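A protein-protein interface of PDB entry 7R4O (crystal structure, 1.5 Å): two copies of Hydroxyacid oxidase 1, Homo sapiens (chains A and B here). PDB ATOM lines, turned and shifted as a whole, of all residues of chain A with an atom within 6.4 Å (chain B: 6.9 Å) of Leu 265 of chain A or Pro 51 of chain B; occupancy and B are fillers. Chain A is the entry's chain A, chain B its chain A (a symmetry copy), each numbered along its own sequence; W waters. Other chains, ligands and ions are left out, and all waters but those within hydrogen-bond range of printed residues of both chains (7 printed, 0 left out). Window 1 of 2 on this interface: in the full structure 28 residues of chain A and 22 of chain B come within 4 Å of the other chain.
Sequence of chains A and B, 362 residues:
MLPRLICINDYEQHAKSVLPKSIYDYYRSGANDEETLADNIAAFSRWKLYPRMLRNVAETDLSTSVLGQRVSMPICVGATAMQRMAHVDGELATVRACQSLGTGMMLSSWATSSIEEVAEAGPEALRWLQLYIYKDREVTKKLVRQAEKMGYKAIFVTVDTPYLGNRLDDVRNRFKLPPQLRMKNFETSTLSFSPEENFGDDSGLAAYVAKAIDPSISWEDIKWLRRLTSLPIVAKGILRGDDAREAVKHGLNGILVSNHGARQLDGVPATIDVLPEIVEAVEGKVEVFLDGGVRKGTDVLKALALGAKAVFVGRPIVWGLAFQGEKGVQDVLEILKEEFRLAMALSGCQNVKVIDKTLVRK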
ATOM      1  N   ALA A  31     -35.807  10.917 -32.062  1.00  0.00           N
ATOM      2  CA  ALA A  31     -35.115  10.288 -30.924  1.00  0.00           C
ATOM      3  C   ALA A  31     -36.097  10.032 -29.777  1.00  0.00           C
ATOM      4  O   ALA A  31     -36.936  10.849 -29.464  1.00  0.00           O
ATOM      5  CB  ALA A  31     -33.970  11.145 -30.447  1.00  0.00           C
ATOM      6  N   ASN A  32     -35.897   8.882 -29.127  1.00  0.00           N
ATOM      7  CA  ASN A  32     -36.613   8.578 -27.866  1.00  0.00           C
ATOM      8  C   ASN A  32     -38.125   8.765 -28.009  1.00  0.00           C
ATOM      9  O   ASN A  32     -38.684   8.170 -28.899  1.00  0.00           O
ATOM     10  CB  ASN A  32     -35.932   9.344 -26.718  1.00  0.00           C
ATOM     11  CG  ASN A  32     -34.454   9.039 -26.597  1.00  0.00           C
ATOM     12  OD1 ASN A  32     -34.068   8.068 -25.958  1.00  0.00           O
ATOM     13  ND2 ASN A  32     -33.624   9.863 -27.204  1.00  0.00           N
ATOM     14  N   THR A  36     -39.489  16.360 -29.445  1.00  0.00           N
ATOM     15  CA  THR A  36     -39.042  17.442 -30.319  1.00  0.00           C
ATOM     16  C   THR A  36     -39.632  17.227 -31.717  1.00  0.00           C
ATOM     17  O   THR A  36     -39.922  18.177 -32.441  1.00  0.00           O
ATOM     18  CB  THR A  36     -37.517  17.510 -30.327  1.00  0.00           C
ATOM     19  OG1 THR A  36     -37.078  17.818 -28.996  1.00  0.00           O
ATOM     20  CG2 THR A  36     -36.967  18.558 -31.265  1.00  0.00           C
ATOM     21  N   ASP A 160     -23.829  18.358 -34.242  1.00  0.00           N
ATOM     22  CA  ASP A 160     -24.704  17.893 -33.136  1.00  0.00           C
ATOM     23  C   ASP A 160     -24.714  16.374 -33.006  1.00  0.00           C
ATOM     24  O   ASP A 160     -25.556  15.841 -32.282  1.00  0.00           O
ATOM     25  CB  ASP A 160     -26.118  18.414 -33.373  1.00  0.00           C
ATOM     26  CG  ASP A 160     -26.751  17.962 -34.681  1.00  0.00           C
ATOM     27  OD1 ASP A 160     -26.219  17.080 -35.365  1.00  0.00           O
ATOM     28  OD2 ASP A 160     -27.851  18.488 -35.009  1.00  0.00           O
ATOM     29  N   GLY A 165     -28.196   9.734 -32.092  1.00  0.00           N
ATOM     30  CA  GLY A 165     -29.367   9.671 -31.235  1.00  0.00           C
ATOM     31  C   GLY A 165     -29.971   8.275 -31.200  1.00  0.00           C
ATOM     32  O   GLY A 165     -29.750   7.448 -32.138  1.00  0.00           O
ATOM     33  N   GLY A 237     -26.614  22.401 -36.876  1.00  0.00           N
ATOM     34  CA  GLY A 237     -27.028  21.790 -35.603  1.00  0.00           C
ATOM     35  C   GLY A 237     -26.826  22.654 -34.403  1.00  0.00           C
ATOM     36  O   GLY A 237     -27.032  22.183 -33.279  1.00  0.00           O
ATOM     37  N   ILE A 238     -26.535  23.920 -34.570  1.00  0.00           N
ATOM     38  CA  ILE A 238     -26.461  24.875 -33.451  1.00  0.00           C
ATOM     39  C   ILE A 238     -27.841  25.222 -32.935  1.00  0.00           C
ATOM     40  O   ILE A 238     -28.745  25.553 -33.731  1.00  0.00           O
ATOM     41  CB  ILE A 238     -25.753  26.143 -33.916  1.00  0.00           C
ATOM     42  CG1 ILE A 238     -24.385  25.841 -34.485  1.00  0.00           C
ATOM     43  CG2 ILE A 238     -25.727  27.210 -32.842  1.00  0.00           C
ATOM     44  CD1 ILE A 238     -23.454  25.401 -33.502  1.00  0.00           C
ATOM     45  N   LEU A 239     -27.984  25.252 -31.612  1.00  0.00           N
ATOM     46  CA  LEU A 239     -29.252  25.569 -30.926  1.00  0.00           C
ATOM     47  C   LEU A 239     -29.096  26.651 -29.871  1.00  0.00           C
ATOM     48  O   LEU A 239     -30.114  27.053 -29.360  1.00  0.00           O
ATOM     49  CB  LEU A 239     -29.847  24.301 -30.304  1.00  0.00           C
ATOM     50  CG  LEU A 239     -30.305  23.246 -31.300  1.00  0.00           C
ATOM     51  CD1 LEU A 239     -30.619  21.934 -30.583  1.00  0.00           C
ATOM     52  CD2 LEU A 239     -31.473  23.736 -32.124  1.00  0.00           C
ATOM     53  N   ARG A 240     -27.874  27.128 -29.644  1.00  0.00           N
ATOM     54  CA  ARG A 240     -27.588  28.142 -28.599  1.00  0.00           C
ATOM     55  C   ARG A 240     -26.909  29.364 -29.225  1.00  0.00           C
ATOM     56  O   ARG A 240     -26.070  29.204 -30.086  1.00  0.00           O
ATOM     57  CB  ARG A 240     -26.638  27.564 -27.549  1.00  0.00           C
ATOM     58  CG  ARG A 240     -27.242  26.492 -26.656  1.00  0.00           C
ATOM     59  CD  ARG A 240     -26.149  25.878 -25.809  1.00  0.00           C
ATOM     60  NE  ARG A 240     -25.553  26.826 -24.881  1.00  0.00           N
ATOM     61  CZ  ARG A 240     -25.750  26.829 -23.568  1.00  0.00           C
ATOM     62  NH1 ARG A 240     -25.152  27.729 -22.813  1.00  0.00           N
ATOM     63  NH2 ARG A 240     -26.538  25.928 -23.009  1.00  0.00           N
ATOM     64  N   ASP A 242     -24.782  31.320 -27.736  1.00  0.00           N
ATOM     65  CA  ASP A 242     -23.337  31.366 -27.405  1.00  0.00           C
ATOM     66  C   ASP A 242     -22.552  30.532 -28.418  1.00  0.00           C
ATOM     67  O   ASP A 242     -21.470  30.960 -28.907  1.00  0.00           O
ATOM     68  CB  ASP A 242     -23.026  31.017 -25.963  1.00  0.00           C
ATOM     69  CG  ASP A 242     -23.561  29.737 -25.381  1.00  0.00           C
ATOM     70  OD1 ASP A 242     -24.048  28.856 -26.161  1.00  0.00           O
ATOM     71  OD2 ASP A 242     -23.402  29.581 -24.149  1.00  0.00           O
ATOM     72  N   ASP A 243     -23.053  29.340 -28.802  1.00  0.00           N
ATOM     73  CA  ASP A 243     -22.389  28.501 -29.816  1.00  0.00           C
ATOM     74  C   ASP A 243     -22.395  29.220 -31.183  1.00  0.00           C
ATOM     75  O   ASP A 243     -21.442  29.094 -31.929  1.00  0.00           O
ATOM     76  CB  ASP A 243     -23.057  27.122 -29.907  1.00  0.00           C
ATOM     77  CG  ASP A 243     -22.659  26.159 -28.819  1.00  0.00           C
ATOM     78  OD1 ASP A 243     -21.765  26.493 -27.999  1.00  0.00           O
ATOM     79  OD2 ASP A 243     -23.236  25.038 -28.823  1.00  0.00           O
ATOM     80  N   ASN A 259     -32.114  20.838 -35.213  1.00  0.00           N
ATOM     81  CA  ASN A 259     -32.071  19.801 -34.167  1.00  0.00           C
ATOM     82  C   ASN A 259     -31.972  18.452 -34.848  1.00  0.00           C
ATOM     83  O   ASN A 259     -32.348  17.422 -34.283  1.00  0.00           O
ATOM     84  CB  ASN A 259     -33.189  19.917 -33.146  1.00  0.00           C
ATOM     85  CG  ASN A 259     -34.555  20.026 -33.762  1.00  0.00           C
ATOM     86  OD1 ASN A 259     -34.809  19.400 -34.826  1.00  0.00           O
ATOM     87  ND2 ASN A 259     -35.447  20.768 -33.136  1.00  0.00           N
ATOM     88  N   ALA A 262     -34.986  16.319 -35.237  1.00  0.00           N
ATOM     89  CA  ALA A 262     -35.438  15.818 -33.931  1.00  0.00           C
ATOM     90  C   ALA A 262     -34.893  14.396 -33.708  1.00  0.00           C
ATOM     91  O   ALA A 262     -35.541  13.650 -32.989  1.00  0.00           O
ATOM     92  CB  ALA A 262     -36.943  15.927 -33.813  1.00  0.00           C
ATOM     93  N   ARG A 263     -33.753  14.052 -34.291  1.00  0.00           N
ATOM     94  CA  ARG A 263     -33.275  12.647 -34.250  1.00  0.00           C
ATOM     95  C   ARG A 263     -32.055  12.487 -33.341  1.00  0.00           C
ATOM     96  O   ARG A 263     -31.543  11.381 -33.261  1.00  0.00           O
ATOM     97  CB  ARG A 263     -32.911  12.217 -35.676  1.00  0.00           C
ATOM     98  CG  ARG A 263     -34.107  12.064 -36.601  1.00  0.00           C
ATOM     99  CD  ARG A 263     -33.681  12.165 -38.051  1.00  0.00           C
ATOM    100  NE  ARG A 263     -33.033  10.985 -38.598  1.00  0.00           N
ATOM    101  CZ  ARG A 263     -33.663   9.891 -39.003  1.00  0.00           C
ATOM    102  NH1 ARG A 263     -34.974   9.798 -38.889  1.00  0.00           N
ATOM    103  NH2 ARG A 263     -32.980   8.886 -39.520  1.00  0.00           N
ATOM    104  N   GLN A 264     -31.637  13.563 -32.686  1.00  0.00           N
ATOM    105  CA  GLN A 264     -30.419  13.502 -31.843  1.00  0.00           C
ATOM    106  C   GLN A 264     -30.832  13.605 -30.366  1.00  0.00           C
ATOM    107  O   GLN A 264     -31.254  12.598 -29.822  1.00  0.00           O
ATOM    108  CB  GLN A 264     -29.449  14.596 -32.279  1.00  0.00           C
ATOM    109  CG  GLN A 264     -28.692  14.236 -33.554  1.00  0.00           C
ATOM    110  CD  GLN A 264     -27.875  12.977 -33.390  1.00  0.00           C
ATOM    111  OE1 GLN A 264     -28.169  11.940 -33.971  1.00  0.00           O
ATOM    112  NE2 GLN A 264     -26.838  13.057 -32.578  1.00  0.00           N
ATOM    113  N   LEU A 265     -30.738  14.805 -29.770  1.00  0.00           N
ATOM    114  CA  LEU A 265     -31.188  14.949 -28.363  1.00  0.00           C
ATOM    115  C   LEU A 265     -32.665  15.292 -28.344  1.00  0.00           C
ATOM    116  O   LEU A 265     -33.073  16.285 -28.946  1.00  0.00           O
ATOM    117  CB  LEU A 265     -30.345  16.019 -27.704  1.00  0.00           C
ATOM    118  CG  LEU A 265     -30.627  16.268 -26.226  1.00  0.00           C
ATOM    119  CD1 LEU A 265     -30.402  15.027 -25.374  1.00  0.00           C
ATOM    120  CD2 LEU A 265     -29.759  17.434 -25.777  1.00  0.00           C
ATOM    121  N   ASP A 266     -33.480  14.409 -27.768  1.00  0.00           N
ATOM    122  CA  ASP A 266     -34.911  14.739 -27.658  1.00  0.00           C
ATOM    123  C   ASP A 266     -35.146  15.678 -26.482  1.00  0.00           C
ATOM    124  O   ASP A 266     -34.454  15.597 -25.457  1.00  0.00           O
ATOM    125  CB  ASP A 266     -35.774  13.479 -27.464  1.00  0.00           C
ATOM    126  CG  ASP A 266     -37.219  13.773 -27.747  1.00  0.00           C
ATOM    127  OD1 ASP A 266     -37.519  14.528 -28.698  1.00  0.00           O
ATOM    128  OD2 ASP A 266     -38.096  13.207 -27.046  1.00  0.00           O
ATOM    129  N   GLY A 267     -36.122  16.538 -26.656  1.00  0.00           N
ATOM    130  CA  GLY A 267     -36.452  17.561 -25.664  1.00  0.00           C
ATOM    131  C   GLY A 267     -35.755  18.867 -25.857  1.00  0.00           C
ATOM    132  O   GLY A 267     -35.899  19.722 -24.978  1.00  0.00           O
ATOM    133  N   VAL A 268     -35.003  19.025 -26.920  1.00  0.00           N
ATOM    134  CA  VAL A 268     -34.562  20.376 -27.329  1.00  0.00           C
ATOM    135  C   VAL A 268     -35.762  21.103 -27.898  1.00  0.00           C
ATOM    136  O   VAL A 268     -36.763  20.488 -28.308  1.00  0.00           O
ATOM    137  CB  VAL A 268     -33.400  20.288 -28.311  1.00  0.00           C
ATOM    138  CG1 VAL A 268     -32.283  19.494 -27.698  1.00  0.00           C
ATOM    139  CG2 VAL A 268     -33.778  19.662 -29.668  1.00  0.00           C
ATOM    140  N   PRO A 269     -35.693  22.439 -27.957  1.00  0.00           N
ATOM    141  CA  PRO A 269     -36.780  23.187 -28.564  1.00  0.00           C
ATOM    142  C   PRO A 269     -36.899  22.960 -30.073  1.00  0.00           C
ATOM    143  O   PRO A 269     -35.985  22.462 -30.736  1.00  0.00           O
ATOM    144  CB  PRO A 269     -36.434  24.643 -28.331  1.00  0.00           C
ATOM    145  CG  PRO A 269     -35.359  24.609 -27.315  1.00  0.00           C
ATOM    146  CD  PRO A 269     -34.597  23.317 -27.524  1.00  0.00           C
ATOM    147  N   LYS B  48     -37.053  22.240 -21.466  1.00  0.00           N
ATOM    148  CA  LYS B  48     -36.369  21.997 -22.744  1.00  0.00           C
ATOM    149  C   LYS B  48     -34.858  22.090 -22.542  1.00  0.00           C
ATOM    150  O   LYS B  48     -34.362  22.842 -21.687  1.00  0.00           O
ATOM    151  CB  LYS B  48     -36.875  22.987 -23.784  1.00  0.00           C
ATOM    152  CG  LYS B  48     -38.370  22.876 -24.083  1.00  0.00           C
ATOM    153  CD  LYS B  48     -38.743  21.539 -24.683  1.00  0.00           C
ATOM    154  CE  LYS B  48     -40.222  21.280 -24.868  1.00  0.00           C
ATOM    155  NZ  LYS B  48     -40.460  19.974 -25.585  1.00  0.00           N
ATOM    156  N   LEU B  49     -34.132  21.320 -23.321  1.00  0.00           N
ATOM    157  CA  LEU B  49     -32.675  21.236 -23.253  1.00  0.00           C
ATOM    158  C   LEU B  49     -32.041  22.117 -24.319  1.00  0.00           C
ATOM    159  O   LEU B  49     -32.503  22.185 -25.458  1.00  0.00           O
ATOM    160  CB  LEU B  49     -32.262  19.785 -23.479  1.00  0.00           C
ATOM    161  CG  LEU B  49     -32.514  18.888 -22.266  1.00  0.00           C
ATOM    162  CD1 LEU B  49     -32.457  17.420 -22.650  1.00  0.00           C
ATOM    163  CD2 LEU B  49     -31.482  19.152 -21.164  1.00  0.00           C
ATOM    164  N   TYR B  50     -30.965  22.766 -23.921  1.00  0.00           N
ATOM    165  CA  TYR B  50     -30.193  23.723 -24.766  1.00  0.00           C
ATOM    166  C   TYR B  50     -28.770  23.232 -24.869  1.00  0.00           C
ATOM    167  O   TYR B  50     -27.894  23.671 -24.083  1.00  0.00           O
ATOM    168  CB  TYR B  50     -30.271  25.124 -24.158  1.00  0.00           C
ATOM    169  CG  TYR B  50     -31.632  25.718 -24.322  1.00  0.00           C
ATOM    170  CD1 TYR B  50     -32.680  25.344 -23.508  1.00  0.00           C
ATOM    171  CD2 TYR B  50     -31.889  26.547 -25.390  1.00  0.00           C
ATOM    172  CE1 TYR B  50     -33.969  25.801 -23.741  1.00  0.00           C
ATOM    173  CE2 TYR B  50     -33.173  27.032 -25.628  1.00  0.00           C
ATOM    174  CZ  TYR B  50     -34.206  26.661 -24.807  1.00  0.00           C
ATOM    175  OH  TYR B  50     -35.483  27.156 -25.004  1.00  0.00           O
ATOM    176  N   PRO B  51     -28.493  22.210 -25.711  1.00  0.00           N
ATOM    177  CA  PRO B  51     -27.215  21.501 -25.733  1.00  0.00           C
ATOM    178  C   PRO B  51     -26.086  22.328 -26.311  1.00  0.00           C
ATOM    179  O   PRO B  51     -26.320  23.130 -27.227  1.00  0.00           O
ATOM    180  CB  PRO B  51     -27.489  20.317 -26.663  1.00  0.00           C
ATOM    181  CG  PRO B  51     -28.557  20.793 -27.566  1.00  0.00           C
ATOM    182  CD  PRO B  51     -29.461  21.592 -26.659  1.00  0.00           C
ATOM    183  N   ARG B  52     -24.915  22.239 -25.698  1.00  0.00           N
ATOM    184  CA  ARG B  52     -23.713  22.812 -26.307  1.00  0.00           C
ATOM    185  C   ARG B  52     -23.077  21.806 -27.254  1.00  0.00           C
ATOM    186  O   ARG B  52     -23.047  20.585 -26.970  1.00  0.00           O
ATOM    187  CB  ARG B  52     -22.692  23.093 -25.211  1.00  0.00           C
ATOM    188  CG  ARG B  52     -23.081  24.264 -24.318  1.00  0.00           C
ATOM    189  CD  ARG B  52     -21.873  24.483 -23.405  1.00  0.00           C
ATOM    190  NE  ARG B  52     -22.099  25.533 -22.449  1.00  0.00           N
ATOM    191  CZ  ARG B  52     -22.695  25.390 -21.273  1.00  0.00           C
ATOM    192  NH1 ARG B  52     -22.790  26.423 -20.439  1.00  0.00           N
ATOM    193  NH2 ARG B  52     -23.200  24.222 -20.939  1.00  0.00           N
ATOM    194  N   MET B  53     -22.551  22.311 -28.368  1.00  0.00           N
ATOM    195  CA  MET B  53     -21.872  21.489 -29.375  1.00  0.00           C
ATOM    196  C   MET B  53     -20.346  21.601 -29.206  1.00  0.00           C
ATOM    197  O   MET B  53     -19.844  22.607 -28.672  1.00  0.00           O
ATOM    198  CB  MET B  53     -22.337  21.930 -30.775  1.00  0.00           C
ATOM    199  CG  MET B  53     -23.859  22.009 -30.938  1.00  0.00           C
ATOM    200  SD  MET B  53     -24.583  20.407 -30.609  1.00  0.00           S
ATOM    201  CE  MET B  53     -26.293  20.874 -30.280  1.00  0.00           C
ATOM    202  N   THR B 298     -32.708  11.810 -20.262  1.00  0.00           N
ATOM    203  CA  THR B 298     -32.874  13.283 -20.287  1.00  0.00           C
ATOM    204  C   THR B 298     -33.525  13.763 -18.999  1.00  0.00           C
ATOM    205  O   THR B 298     -33.320  14.923 -18.639  1.00  0.00           O
ATOM    206  CB  THR B 298     -33.623  13.750 -21.538  1.00  0.00           C
ATOM    207  OG1 THR B 298     -34.800  12.935 -21.696  1.00  0.00           O
ATOM    208  CG2 THR B 298     -32.760  13.631 -22.785  1.00  0.00           C
ATOM    209  N   LEU B 301     -30.660  14.258 -16.648  1.00  0.00           N
ATOM    210  CA  LEU B 301     -29.901  15.447 -17.043  1.00  0.00           C
ATOM    211  C   LEU B 301     -30.628  16.714 -16.597  1.00  0.00           C
ATOM    212  O   LEU B 301     -29.990  17.637 -16.084  1.00  0.00           O
ATOM    213  CB  LEU B 301     -29.671  15.381 -18.547  1.00  0.00           C
ATOM    214  CG  LEU B 301     -28.872  16.539 -19.133  1.00  0.00           C
ATOM    215  CD1 LEU B 301     -27.450  16.543 -18.596  1.00  0.00           C
ATOM    216  CD2 LEU B 301     -28.814  16.446 -20.664  1.00  0.00           C
ATOM    217  N   GLU B 339     -28.862   5.837 -21.457  1.00  0.00           N
ATOM    218  CA  GLU B 339     -29.623   7.029 -21.923  1.00  0.00           C
ATOM    219  C   GLU B 339     -28.993   8.266 -21.306  1.00  0.00           C
ATOM    220  O   GLU B 339     -28.899   9.307 -21.967  1.00  0.00           O
ATOM    221  CB  GLU B 339     -31.085   6.947 -21.526  1.00  0.00           C
ATOM    222  CG  GLU B 339     -31.917   5.879 -22.284  1.00  0.00           C
ATOM    223  CD  GLU B 339     -33.397   6.146 -22.137  1.00  0.00           C
ATOM    224  OE1 GLU B 339     -33.796   7.282 -21.674  1.00  0.00           O
ATOM    225  OE2 GLU B 339     -34.225   5.261 -22.597  1.00  0.00           O
ATOM    226  N   LEU B 342     -25.727   9.143 -23.107  1.00  0.00           N
ATOM    227  CA  LEU B 342     -25.989   9.731 -24.424  1.00  0.00           C
ATOM    228  C   LEU B 342     -26.471  11.171 -24.252  1.00  0.00           C
ATOM    229  O   LEU B 342     -26.030  12.023 -24.986  1.00  0.00           O
ATOM    230  CB  LEU B 342     -26.949   8.877 -25.200  1.00  0.00           C
ATOM    231  CG  LEU B 342     -27.225   9.370 -26.608  1.00  0.00           C
ATOM    232  CD1 LEU B 342     -25.945   9.377 -27.427  1.00  0.00           C
ATOM    233  CD2 LEU B 342     -28.267   8.487 -27.249  1.00  0.00           C
ATOM    234  N   ALA B 343     -27.374  11.423 -23.323  1.00  0.00           N
ATOM    235  CA  ALA B 343     -27.927  12.771 -23.123  1.00  0.00           C
ATOM    236  C   ALA B 343     -26.824  13.712 -22.702  1.00  0.00           C
ATOM    237  O   ALA B 343     -26.737  14.831 -23.236  1.00  0.00           O
ATOM    238  CB  ALA B 343     -29.025  12.740 -22.109  1.00  0.00           C
ATOM    239  N   MET B 344     -25.932  13.254 -21.825  1.00  0.00           N
ATOM    240  CA  MET B 344     -24.784  14.083 -21.411  1.00  0.00           C
ATOM    241  C   MET B 344     -23.939  14.396 -22.651  1.00  0.00           C
ATOM    242  O   MET B 344     -23.576  15.563 -22.922  1.00  0.00           O
ATOM    243  CB  MET B 344     -23.944  13.279 -20.431  1.00  0.00           C
ATOM    244  CG  MET B 344     -24.458  13.312 -19.073  1.00  0.00           C
ATOM    245  SD  MET B 344     -23.277  12.548 -17.907  1.00  0.00           S
ATOM    246  CE  MET B 344     -21.861  13.561 -18.026  1.00  0.00           C
ATOM    247  N   ALA B 345     -23.608  13.390 -23.436  1.00  0.00           N
ATOM    248  CA  ALA B 345     -22.689  13.551 -24.581  1.00  0.00           C
ATOM    249  C   ALA B 345     -23.316  14.494 -25.612  1.00  0.00           C
ATOM    250  O   ALA B 345     -22.673  15.461 -26.070  1.00  0.00           O
ATOM    251  CB  ALA B 345     -22.365  12.213 -25.168  1.00  0.00           C
ATOM    252  N   LEU B 346     -24.594  14.311 -25.910  1.00  0.00           N
ATOM    253  CA  LEU B 346     -25.243  15.160 -26.947  1.00  0.00           C
ATOM    254  C   LEU B 346     -25.408  16.597 -26.456  1.00  0.00           C
ATOM    255  O   LEU B 346     -25.556  17.483 -27.261  1.00  0.00           O
ATOM    256  CB  LEU B 346     -26.590  14.556 -27.355  1.00  0.00           C
ATOM    257  CG  LEU B 346     -26.507  13.187 -28.023  1.00  0.00           C
ATOM    258  CD1 LEU B 346     -27.884  12.721 -28.466  1.00  0.00           C
ATOM    259  CD2 LEU B 346     -25.551  13.221 -29.203  1.00  0.00           C
ATOM    260  N   SER B 347     -25.367  16.793 -25.134  1.00  0.00           N
ATOM    261  CA  SER B 347     -25.524  18.157 -24.557  1.00  0.00           C
ATOM    262  C   SER B 347     -24.161  18.832 -24.369  1.00  0.00           C
ATOM    263  O   SER B 347     -24.130  19.971 -23.877  1.00  0.00           O
ATOM    264  CB  SER B 347     -26.313  18.107 -23.268  1.00  0.00           C
ATOM    265  OG  SER B 347     -25.646  17.334 -22.286  1.00  0.00           O
ATOM    266  N   GLY B 348     -23.074  18.086 -24.586  1.00  0.00           N
ATOM    267  CA  GLY B 348     -21.712  18.663 -24.456  1.00  0.00           C
ATOM    268  C   GLY B 348     -21.109  18.495 -23.079  1.00  0.00           C
ATOM    269  O   GLY B 348     -20.174  19.199 -22.781  1.00  0.00           O
ATOM    270  N   THR B 358     -27.737  26.508 -17.493  1.00  0.00           N
ATOM    271  CA  THR B 358     -28.034  27.040 -18.858  1.00  0.00           C
ATOM    272  C   THR B 358     -28.449  25.917 -19.811  1.00  0.00           C
ATOM    273  O   THR B 358     -29.004  26.214 -20.872  1.00  0.00           O
ATOM    274  CB  THR B 358     -26.889  27.803 -19.536  1.00  0.00           C
ATOM    275  OG1 THR B 358     -25.921  26.875 -20.037  1.00  0.00           O
ATOM    276  CG2 THR B 358     -26.301  28.868 -18.630  1.00  0.00           C
ATOM    277  N   LEU B 359     -28.294  24.660 -19.405  1.00  0.00           N
ATOM    278  CA  LEU B 359     -28.775  23.551 -20.256  1.00  0.00           C
ATOM    279  C   LEU B 359     -30.290  23.469 -20.286  1.00  0.00           C
ATOM    280  O   LEU B 359     -30.806  22.730 -21.172  1.00  0.00           O
ATOM    281  CB  LEU B 359     -28.223  22.229 -19.763  1.00  0.00           C
ATOM    282  CG  LEU B 359     -26.757  22.029 -19.982  1.00  0.00           C
ATOM    283  CD1 LEU B 359     -26.321  20.743 -19.294  1.00  0.00           C
ATOM    284  CD2 LEU B 359     -26.399  21.985 -21.454  1.00  0.00           C
HETATM  285  O   HOH W   1     -25.834  24.749 -29.581  1.00  0.00           O
HETATM  286  O   HOH W   2     -39.480  20.441 -28.192  1.00  0.00           O
HETATM  287  O   HOH W   3     -19.653  24.951 -27.479  1.00  0.00           O
HETATM  288  O   HOH W   4     -26.754  17.109 -29.963  1.00  0.00           O
HETATM  289  O   HOH W   5     -20.929  27.870 -23.685  1.00  0.00           O
HETATM  290  O   HOH W   6     -36.039  15.540 -23.135  1.00  0.00           O
HETATM  291  O   HOH W   7     -36.032   6.626 -24.385  1.00  0.00           O
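Hydrophobic or aromatic side chains of chain A that line the printed part of chain B: Leu 239, Leu 265, Val 268 and Pro 269.
Of the 18 printed residues of chain B, 9 touch a printed residue of chain A.
Hydrophobic or aromatic side chains of chain B that line the printed part of chain A: Leu 49, Tyr 50, Pro 51, Met 53 and Leu 346.
Among the printed residues, 22 pairs touch across the chains.
Among the printed residues, no Asp or Glu carboxylate lies within 4 Å of a Lys or Arg side-chain nitrogen of the other chain.
The side-chain carboxylate of Asp 266 of chain A is in hydrogen-bond range of the backbone NH of Thr 36 of chain A (2.8 Å).
N of Gly 165 of chain A sits at hydrogen-bond distance from OE1 of Gln 264 of chain A, 2.9 Å away.
The side-chain amide nitrogen (NE2) of Gln 264 of chain A lies within hydrogen-bond range of the backbone carbonyl oxygen (O) of Asp 160 of chain A, at 3.1 Å.
No position is printed for both chains.
Of the 22 pairs that touch across the chains among the printed residues, none has its exchanged pair printed and touching as well.
The backbone carbonyl oxygen of Gly 267 of chain A is in hydrogen-bond range of the backbone NH of Leu 49 of chain B, 2.9 Å away.
The guanidinium group of Arg 240 of chain A lies within hydrogen-bond range of the side-chain hydroxyl of Thr 358 of chain B, 3.0 Å away.
NH2 of Arg 240 of chain A lies within hydrogen-bond range of O of Tyr 50 of chain B.
OD2 of Asp 243 of chain A lies within hydrogen-bond range of N of Met 53 of chain B, at 2.8 Å.
Water W1 lies within hydrogen-bond range of the side-chain carboxylate (OD2) of Asp 243 of chain A, the backbone carbonyl oxygen (O) of Pro 51 of chain B, the backbone NH (N) of Leu 239 of chain A and the backbone NH (N) of Arg 240 of chain A.
Water W4 lies within hydrogen-bond range of O of Asp 160 of chain A (2.9 Å) and O of Leu 346 of chain B (3.0 Å).
Pro 51 of chain B touches five residues of chain A.
Of the printed residues of chain B, Gly 237 of chain A touches Met 53.
Printed residues of chain A within 4 Å of Leu 49 of chain B: Asp 266 (3.9 Å), Gly 267 (2.9 Å), Val 268 (3.3 Å) and Pro 269 (3.2 Å).
Printed residues of chain B within 4 Å of Pro 269 of chain A: Leu 49 and Tyr 50.
Of the printed residues of chain A, Tyr 50 of chain B touches Arg 240 and Pro 269.
Asp 242 of chain A touches none of the printed residues of chain B.
The nearest residue of chain A that does not touch Pro 51 of chain B is Pro 269 of chain A (5.5 Å).
The nearest printed residue of chain B that does not touch Gln 264 of chain A is Leu 342 of chain B (5.7 Å).
Among the printed residues, pairs that only touch across the chains: Arg 240 of chain A with Pro 51 of chain B (3.1 Å), Pro 269 of chain A with Leu 49 of chain B (3.2 Å), Gly 267 of chain A with Lys 48 of chain B (3.2 Å), Val 268 of chain A with Leu 49 of chain B (3.3 Å), Gly 237 of chain A with Met 53 of chain B (3.4 Å), Asp 243 of chain A with Arg 52 of chain B (3.4 Å), Pro 269 of chain A with Tyr 50 of chain B (3.4 Å), Asp 160 of chain A with Met 53 of chain B (3.6 Å), Arg 240 of chain A with Arg 52 of chain B (3.6 Å), Gln 264 of chain A with Leu 346 of chain B (3.6 Å), Val 268 of chain A with Pro 51 of chain B (3.7 Å), Asp 266 of chain A with Thr 298 of chain B (3.7 Å), Leu 265 of chain A with Leu 346 of chain B (3.8 Å), Leu 265 of chain A with Thr 298 of chain B (3.8 Å), Leu 265 of chain A with Pro 51 of chain B (3.8 Å), Leu 239 of chain A with Pro 51 of chain B (3.8 Å), Asp 266 of chain A with Leu 49 of chain B (3.9 Å) and Asp 243 of chain A with Pro 51 of chain B (3.96 Å).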
